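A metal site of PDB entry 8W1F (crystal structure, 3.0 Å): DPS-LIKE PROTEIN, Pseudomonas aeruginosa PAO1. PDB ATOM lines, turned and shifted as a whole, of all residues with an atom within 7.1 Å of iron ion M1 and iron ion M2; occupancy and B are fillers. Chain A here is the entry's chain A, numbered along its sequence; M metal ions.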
ATOM      1  N   ALA A  43      25.505  20.021  12.897  1.00  0.00           N
ATOM      2  CA  ALA A  43      24.533  19.828  13.970  1.00  0.00           C
ATOM      3  C   ALA A  43      23.415  18.904  13.500  1.00  0.00           C
ATOM      4  O   ALA A  43      22.993  18.010  14.232  1.00  0.00           O
ATOM      5  CB  ALA A  43      23.977  21.174  14.417  1.00  0.00           C
ATOM      6  N   THR A  46      24.538  15.408  13.682  1.00  0.00           N
ATOM      7  CA  THR A  46      24.554  14.998  15.082  1.00  0.00           C
ATOM      8  C   THR A  46      23.163  14.642  15.580  1.00  0.00           C
ATOM      9  O   THR A  46      22.975  13.623  16.259  1.00  0.00           O
ATOM     10  CB  THR A  46      25.154  16.119  15.928  1.00  0.00           C
ATOM     11  OG1 THR A  46      26.470  16.413  15.441  1.00  0.00           O
ATOM     12  CG2 THR A  46      25.231  15.697  17.381  1.00  0.00           C
ATOM     13  N   GLU A  47      22.163  15.464  15.242  1.00  0.00           N
ATOM     14  CA  GLU A  47      20.809  15.188  15.713  1.00  0.00           C
ATOM     15  C   GLU A  47      20.270  13.894  15.144  1.00  0.00           C
ATOM     16  O   GLU A  47      19.578  13.152  15.841  1.00  0.00           O
ATOM     17  CB  GLU A  47      19.874  16.359  15.385  1.00  0.00           C
ATOM     18  CG  GLU A  47      20.336  17.680  16.017  1.00  0.00           C
ATOM     19  CD  GLU A  47      20.332  17.634  17.548  1.00  0.00           C
ATOM     20  OE1 GLU A  47      19.520  16.873  18.118  1.00  0.00           O
ATOM     21  OE2 GLU A  47      21.146  18.329  18.181  1.00  0.00           O
ATOM     22  N   CYS A  50      21.948  10.917  16.986  1.00  0.00           N
ATOM     23  CA  CYS A  50      21.379  10.760  18.320  1.00  0.00           C
ATOM     24  C   CYS A  50      19.946  10.243  18.247  1.00  0.00           C
ATOM     25  O   CYS A  50      19.519   9.475  19.114  1.00  0.00           O
ATOM     26  CB  CYS A  50      21.481  12.089  19.087  1.00  0.00           C
ATOM     27  SG  CYS A  50      23.186  12.552  19.659  1.00  0.00           S
ATOM     28  N   TYR A  54      18.915   6.730  20.180  1.00  0.00           N
ATOM     29  CA  TYR A  54      17.871   6.680  21.203  1.00  0.00           C
ATOM     30  C   TYR A  54      16.767   5.713  20.802  1.00  0.00           C
ATOM     31  O   TYR A  54      16.228   4.999  21.642  1.00  0.00           O
ATOM     32  CB  TYR A  54      17.327   8.077  21.431  1.00  0.00           C
ATOM     33  CG  TYR A  54      18.017   8.901  22.489  1.00  0.00           C
ATOM     34  CD1 TYR A  54      18.015   8.521  23.824  1.00  0.00           C
ATOM     35  CD2 TYR A  54      18.615  10.098  22.160  1.00  0.00           C
ATOM     36  CE1 TYR A  54      18.611   9.302  24.802  1.00  0.00           C
ATOM     37  CE2 TYR A  54      19.200  10.900  23.135  1.00  0.00           C
ATOM     38  CZ  TYR A  54      19.193  10.496  24.447  1.00  0.00           C
ATOM     39  OH  TYR A  54      19.778  11.301  25.413  1.00  0.00           O
ATOM     40  N   HIS A  76      13.465  11.648  24.281  1.00  0.00           N
ATOM     41  CA  HIS A  76      14.647  12.329  23.785  1.00  0.00           C
ATOM     42  C   HIS A  76      14.812  12.126  22.283  1.00  0.00           C
ATOM     43  O   HIS A  76      15.071  13.077  21.555  1.00  0.00           O
ATOM     44  CB  HIS A  76      15.893  11.851  24.538  1.00  0.00           C
ATOM     45  CG  HIS A  76      15.901  12.258  25.979  1.00  0.00           C
ATOM     46  ND1 HIS A  76      17.017  12.109  26.785  1.00  0.00           N
ATOM     47  CD2 HIS A  76      14.935  12.795  26.769  1.00  0.00           C
ATOM     48  CE1 HIS A  76      16.726  12.536  28.008  1.00  0.00           C
ATOM     49  NE2 HIS A  76      15.468  12.958  28.022  1.00  0.00           N
ATOM     50  N   GLN A  79      12.679  14.515  20.464  1.00  0.00           N
ATOM     51  CA  GLN A  79      13.200  15.875  20.589  1.00  0.00           C
ATOM     52  C   GLN A  79      14.416  16.084  19.704  1.00  0.00           C
ATOM     53  O   GLN A  79      14.572  17.149  19.099  1.00  0.00           O
ATOM     54  CB  GLN A  79      13.534  16.177  22.058  1.00  0.00           C
ATOM     55  CG  GLN A  79      12.276  16.523  22.841  1.00  0.00           C
ATOM     56  CD  GLN A  79      12.399  16.357  24.336  1.00  0.00           C
ATOM     57  OE1 GLN A  79      13.435  15.984  24.870  1.00  0.00           O
ATOM     58  NE2 GLN A  79      11.296  16.590  25.033  1.00  0.00           N
ATOM     59  N   GLU A  80      15.279  15.080  19.576  1.00  0.00           N
ATOM     60  CA  GLU A  80      16.430  15.227  18.691  1.00  0.00           C
ATOM     61  C   GLU A  80      15.977  15.482  17.260  1.00  0.00           C
ATOM     62  O   GLU A  80      16.608  16.252  16.528  1.00  0.00           O
ATOM     63  CB  GLU A  80      17.320  13.995  18.736  1.00  0.00           C
ATOM     64  CG  GLU A  80      17.864  13.630  20.101  1.00  0.00           C
ATOM     65  CD  GLU A  80      18.564  14.748  20.810  1.00  0.00           C
ATOM     66  OE1 GLU A  80      18.974  15.744  20.167  1.00  0.00           O
ATOM     67  OE2 GLU A  80      18.744  14.610  22.024  1.00  0.00           O
ATOM     68  N   MET A  81      14.906  14.812  16.832  1.00  0.00           N
ATOM     69  CA  MET A  81      14.403  15.032  15.480  1.00  0.00           C
ATOM     70  C   MET A  81      13.804  16.431  15.310  1.00  0.00           C
ATOM     71  O   MET A  81      13.899  17.001  14.221  1.00  0.00           O
ATOM     72  CB  MET A  81      13.399  13.954  15.134  1.00  0.00           C
ATOM     73  CG  MET A  81      13.137  13.841  13.657  1.00  0.00           C
ATOM     74  SD  MET A  81      14.429  12.996  12.769  1.00  0.00           S
ATOM     75  CE  MET A  81      14.395  14.037  11.315  1.00  0.00           C
ATOM     76  N   GLN A  82      13.177  16.990  16.362  1.00  0.00           N
ATOM     77  CA  GLN A  82      12.699  18.374  16.281  1.00  0.00           C
ATOM     78  C   GLN A  82      13.860  19.323  16.060  1.00  0.00           C
ATOM     79  O   GLN A  82      13.772  20.263  15.261  1.00  0.00           O
ATOM     80  CB  GLN A  82      11.953  18.766  17.535  1.00  0.00           C
ATOM     81  CG  GLN A  82      10.604  18.137  17.691  1.00  0.00           C
ATOM     82  CD  GLN A  82      10.072  18.197  19.128  1.00  0.00           C
ATOM     83  OE1 GLN A  82      10.740  18.718  20.035  1.00  0.00           O
ATOM     84  NE2 GLN A  82       8.874  17.671  19.329  1.00  0.00           N
ATOM     85  N   HIS A  83      14.962  19.106  16.790  1.00  0.00           N
ATOM     86  CA  HIS A  83      16.157  19.902  16.557  1.00  0.00           C
ATOM     87  C   HIS A  83      16.648  19.757  15.135  1.00  0.00           C
ATOM     88  O   HIS A  83      17.070  20.728  14.504  1.00  0.00           O
ATOM     89  CB  HIS A  83      17.252  19.478  17.534  1.00  0.00           C
ATOM     90  CG  HIS A  83      16.847  19.566  18.969  1.00  0.00           C
ATOM     91  ND1 HIS A  83      17.484  18.840  19.955  1.00  0.00           N
ATOM     92  CD2 HIS A  83      15.869  20.276  19.572  1.00  0.00           C
ATOM     93  CE1 HIS A  83      16.897  19.106  21.118  1.00  0.00           C
ATOM     94  NE2 HIS A  83      15.920  19.975  20.914  1.00  0.00           N
ATOM     95  N   ALA A  84      16.616  18.529  14.617  1.00  0.00           N
ATOM     96  CA  ALA A  84      17.017  18.307  13.231  1.00  0.00           C
ATOM     97  C   ALA A  84      16.164  19.148  12.294  1.00  0.00           C
ATOM     98  O   ALA A  84      16.671  19.766  11.353  1.00  0.00           O
ATOM     99  CB  ALA A  84      16.913  16.835  12.883  1.00  0.00           C
ATOM    100  N   LEU A  87      17.079  22.859  12.504  1.00  0.00           N
ATOM    101  CA  LEU A  87      18.325  23.110  11.805  1.00  0.00           C
ATOM    102  C   LEU A  87      18.160  23.021  10.290  1.00  0.00           C
ATOM    103  O   LEU A  87      18.670  23.866   9.552  1.00  0.00           O
ATOM    104  CB  LEU A  87      19.378  22.120  12.290  1.00  0.00           C
ATOM    105  CG  LEU A  87      19.734  22.147  13.778  1.00  0.00           C
ATOM    106  CD1 LEU A  87      20.425  20.845  14.130  1.00  0.00           C
ATOM    107  CD2 LEU A  87      20.612  23.346  14.083  1.00  0.00           C
ATOM    108  N   ASN A 126      24.464   7.812  25.912  1.00  0.00           N
ATOM    109  CA  ASN A 126      23.607   8.973  25.738  1.00  0.00           C
ATOM    110  C   ASN A 126      24.137  10.155  26.520  1.00  0.00           C
ATOM    111  O   ASN A 126      24.188  11.273  26.009  1.00  0.00           O
ATOM    112  CB  ASN A 126      22.172   8.632  26.130  1.00  0.00           C
ATOM    113  CG  ASN A 126      21.534   7.653  25.170  1.00  0.00           C
ATOM    114  OD1 ASN A 126      21.848   7.662  23.983  1.00  0.00           O
ATOM    115  ND2 ASN A 126      20.640   6.824  25.671  1.00  0.00           N
ATOM    116  N   ALA A 129      26.960  11.728  24.729  1.00  0.00           N
ATOM    117  CA  ALA A 129      26.543  12.498  23.568  1.00  0.00           C
ATOM    118  C   ALA A 129      25.995  13.856  23.955  1.00  0.00           C
ATOM    119  O   ALA A 129      26.298  14.861  23.320  1.00  0.00           O
ATOM    120  CB  ALA A 129      25.482  11.725  22.774  1.00  0.00           C
ATOM    121  N   GLU A 130      25.183  13.897  25.001  1.00  0.00           N
ATOM    122  CA  GLU A 130      24.593  15.159  25.429  1.00  0.00           C
ATOM    123  C   GLU A 130      25.676  16.151  25.829  1.00  0.00           C
ATOM    124  O   GLU A 130      25.617  17.338  25.464  1.00  0.00           O
ATOM    125  CB  GLU A 130      23.619  14.912  26.587  1.00  0.00           C
ATOM    126  CG  GLU A 130      22.475  13.934  26.256  1.00  0.00           C
ATOM    127  CD  GLU A 130      21.563  14.445  25.165  1.00  0.00           C
ATOM    128  OE1 GLU A 130      21.710  15.630  24.813  1.00  0.00           O
ATOM    129  OE2 GLU A 130      20.727  13.659  24.666  1.00  0.00           O
ATOM    130  N   ALA A 133      27.384  17.558  22.770  1.00  0.00           N
ATOM    131  CA  ALA A 133      26.544  18.539  22.096  1.00  0.00           C
ATOM    132  C   ALA A 133      26.548  19.857  22.852  1.00  0.00           C
ATOM    133  O   ALA A 133      26.629  20.929  22.245  1.00  0.00           O
ATOM    134  CB  ALA A 133      25.118  18.027  21.982  1.00  0.00           C
ATOM    135  N   TYR A 137      27.539  23.329  21.075  1.00  0.00           N
ATOM    136  CA  TYR A 137      26.558  24.374  20.851  1.00  0.00           C
ATOM    137  C   TYR A 137      26.906  25.622  21.640  1.00  0.00           C
ATOM    138  O   TYR A 137      26.601  26.732  21.191  1.00  0.00           O
ATOM    139  CB  TYR A 137      25.171  23.840  21.169  1.00  0.00           C
ATOM    140  CG  TYR A 137      24.769  22.686  20.254  1.00  0.00           C
ATOM    141  CD1 TYR A 137      25.402  22.488  19.025  1.00  0.00           C
ATOM    142  CD2 TYR A 137      23.779  21.781  20.615  1.00  0.00           C
ATOM    143  CE1 TYR A 137      25.051  21.449  18.199  1.00  0.00           C
ATOM    144  CE2 TYR A 137      23.429  20.746  19.780  1.00  0.00           C
ATOM    145  CZ  TYR A 137      24.072  20.580  18.577  1.00  0.00           C
ATOM    146  OH  TYR A 137      23.754  19.548  17.723  1.00  0.00           O
ATOM    147  N   ILE A 158      18.076  24.725  21.444  1.00  0.00           N
ATOM    148  CA  ILE A 158      18.538  23.351  21.397  1.00  0.00           C
ATOM    149  C   ILE A 158      19.474  23.043  22.560  1.00  0.00           C
ATOM    150  O   ILE A 158      19.357  22.012  23.227  1.00  0.00           O
ATOM    151  CB  ILE A 158      19.230  23.061  20.053  1.00  0.00           C
ATOM    152  CG1 ILE A 158      18.193  23.071  18.924  1.00  0.00           C
ATOM    153  CG2 ILE A 158      20.002  21.741  20.138  1.00  0.00           C
ATOM    154  CD1 ILE A 158      18.812  23.042  17.574  1.00  0.00           C
ATOM    155  N   LEU A 159      20.433  23.948  22.824  1.00  0.00           N
ATOM    156  CA  LEU A 159      21.355  23.764  23.932  1.00  0.00           C
ATOM    157  C   LEU A 159      20.607  23.472  25.216  1.00  0.00           C
ATOM    158  O   LEU A 159      20.926  22.539  25.956  1.00  0.00           O
ATOM    159  CB  LEU A 159      22.219  25.026  24.100  1.00  0.00           C
ATOM    160  CG  LEU A 159      23.061  25.118  25.384  1.00  0.00           C
ATOM    161  CD1 LEU A 159      24.093  24.006  25.503  1.00  0.00           C
ATOM    162  CD2 LEU A 159      23.731  26.455  25.453  1.00  0.00           C
ATOM    163  N   GLN A 161      17.779  22.223  25.744  1.00  0.00           N
ATOM    164  CA  GLN A 161      17.214  20.872  25.731  1.00  0.00           C
ATOM    165  C   GLN A 161      18.284  19.818  25.968  1.00  0.00           C
ATOM    166  O   GLN A 161      18.034  18.830  26.657  1.00  0.00           O
ATOM    167  CB  GLN A 161      16.531  20.597  24.396  1.00  0.00           C
ATOM    168  CG  GLN A 161      15.718  19.331  24.405  1.00  0.00           C
ATOM    169  CD  GLN A 161      14.238  19.621  24.444  1.00  0.00           C
ATOM    170  OE1 GLN A 161      13.655  20.197  23.492  1.00  0.00           O
ATOM    171  NE2 GLN A 161      13.600  19.248  25.555  1.00  0.00           N
ATOM    172  N   GLU A 162      19.469  20.005  25.368  1.00  0.00           N
ATOM    173  CA  GLU A 162      20.557  19.041  25.580  1.00  0.00           C
ATOM    174  C   GLU A 162      21.013  19.051  27.034  1.00  0.00           C
ATOM    175  O   GLU A 162      21.352  17.996  27.587  1.00  0.00           O
ATOM    176  CB  GLU A 162      21.752  19.349  24.673  1.00  0.00           C
ATOM    177  CG  GLU A 162      21.453  19.479  23.183  1.00  0.00           C
ATOM    178  CD  GLU A 162      20.670  18.331  22.610  1.00  0.00           C
ATOM    179  OE1 GLU A 162      20.026  17.615  23.377  1.00  0.00           O
ATOM    180  OE2 GLU A 162      20.704  18.141  21.370  1.00  0.00           O
ATOM    181  N   GLU A 163      21.028  20.226  27.681  1.00  0.00           N
ATOM    182  CA  GLU A 163      21.370  20.270  29.099  1.00  0.00           C
ATOM    183  C   GLU A 163      20.352  19.468  29.924  1.00  0.00           C
ATOM    184  O   GLU A 163      20.718  18.744  30.850  1.00  0.00           O
ATOM    185  CB  GLU A 163      21.452  21.713  29.608  1.00  0.00           C
ATOM    186  CG  GLU A 163      22.547  22.620  28.990  1.00  0.00           C
ATOM    187  CD  GLU A 163      22.864  23.859  29.884  1.00  0.00           C
ATOM    188  OE1 GLU A 163      22.722  23.728  31.114  1.00  0.00           O
ATOM    189  OE2 GLU A 163      23.242  24.954  29.361  1.00  0.00           O
ATOM    190  N   GLU A 164      19.077  19.576  29.573  1.00  0.00           N
ATOM    191  CA  GLU A 164      18.052  18.768  30.241  1.00  0.00           C
ATOM    192  C   GLU A 164      18.261  17.281  29.983  1.00  0.00           C
ATOM    193  O   GLU A 164      18.086  16.459  30.885  1.00  0.00           O
ATOM    194  CB  GLU A 164      16.668  19.233  29.782  1.00  0.00           C
ATOM    195  CG  GLU A 164      15.484  18.365  30.225  1.00  0.00           C
ATOM    196  CD  GLU A 164      14.145  18.955  29.793  1.00  0.00           C
ATOM    197  OE1 GLU A 164      14.049  20.187  29.612  1.00  0.00           O
ATOM    198  OE2 GLU A 164      13.201  18.163  29.615  1.00  0.00           O
ATOM    199  N   HIS A 165      18.622  16.908  28.746  1.00  0.00           N
ATOM    200  CA  HIS A 165      18.850  15.490  28.454  1.00  0.00           C
ATOM    201  C   HIS A 165      20.013  14.958  29.287  1.00  0.00           C
ATOM    202  O   HIS A 165      19.929  13.853  29.835  1.00  0.00           O
ATOM    203  CB  HIS A 165      19.153  15.285  26.971  1.00  0.00           C
ATOM    204  CG  HIS A 165      17.987  15.503  26.061  1.00  0.00           C
ATOM    205  ND1 HIS A 165      18.111  15.620  24.702  1.00  0.00           N
ATOM    206  CD2 HIS A 165      16.659  15.616  26.326  1.00  0.00           C
ATOM    207  CE1 HIS A 165      16.924  15.807  24.162  1.00  0.00           C
ATOM    208  NE2 HIS A 165      16.019  15.808  25.118  1.00  0.00           N
ATOM    209  N   ALA A 166      21.085  15.736  29.391  1.00  0.00           N
ATOM    210  CA  ALA A 166      22.219  15.328  30.212  1.00  0.00           C
ATOM    211  C   ALA A 166      21.802  15.183  31.672  1.00  0.00           C
ATOM    212  O   ALA A 166      22.213  14.230  32.342  1.00  0.00           O
ATOM    213  CB  ALA A 166      23.358  16.327  30.046  1.00  0.00           C
HETATM  214 FE    FE M   1      19.890  15.512  23.400  1.00  0.00          FE
HETATM  215 FE    FE M   2      19.368  17.656  19.963  1.00  0.00          FE
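OE2 of Glu 80 is bound to iron ion M1 (2.0 Å). Iron ion M1 is bound by the side-chain carboxylate (OE1) of Glu 162. ND1 of His 165 binds iron ion M1 (2.2 Å). Iron ion M1 is bound by OE1 of Glu 130. OE2 of Glu 130 binds iron ion M1 (2.4 Å).
Iron ion M2 is bound by the side-chain carboxylate (OE1) of Glu 80 (2.0 Å), the side-chain carboxylate (OE2) of Glu 162 (2.0 Å), the side-chain carboxylate (OE1) of Glu 47 (2.0 Å) and a ring nitrogen (ND1) of His 83 (2.2 Å). Iron ion M2 has four donor atoms within binding distance. Slightly farther from iron ion M2 lies the side-chain carboxylate (OE2) of Glu 47 (2.6 Å).
OE1 of Gln 79 sits at hydrogen-bond distance from NE2 of His 165 (2.6 Å). The side-chain carboxylate (OE2) of Glu 47 sits at hydrogen-bond distance from the side-chain hydroxyl (OH) of Tyr 137. NE2 of His 83 lies within hydrogen-bond range of OE1 of Gln 161 (3.4 Å). ND1 of His 83 lies close to O of Gln 79 (3.5 Å). OE2 of Glu 130 lies close to OH of Tyr 54 (2.6 Å).
Within 4 Å of iron ion M1: Glu 80, Glu 130, Glu 162 and His 165. Along chain A the residues within 4 Å of iron ion M1 span positions 80 to 165.
Within 4 Å of iron ion M2: Glu 47, Glu 80, His 83 and Glu 162. The nearest printed residue that does not touch iron ion M2 is Ile 158 (4.1 Å).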
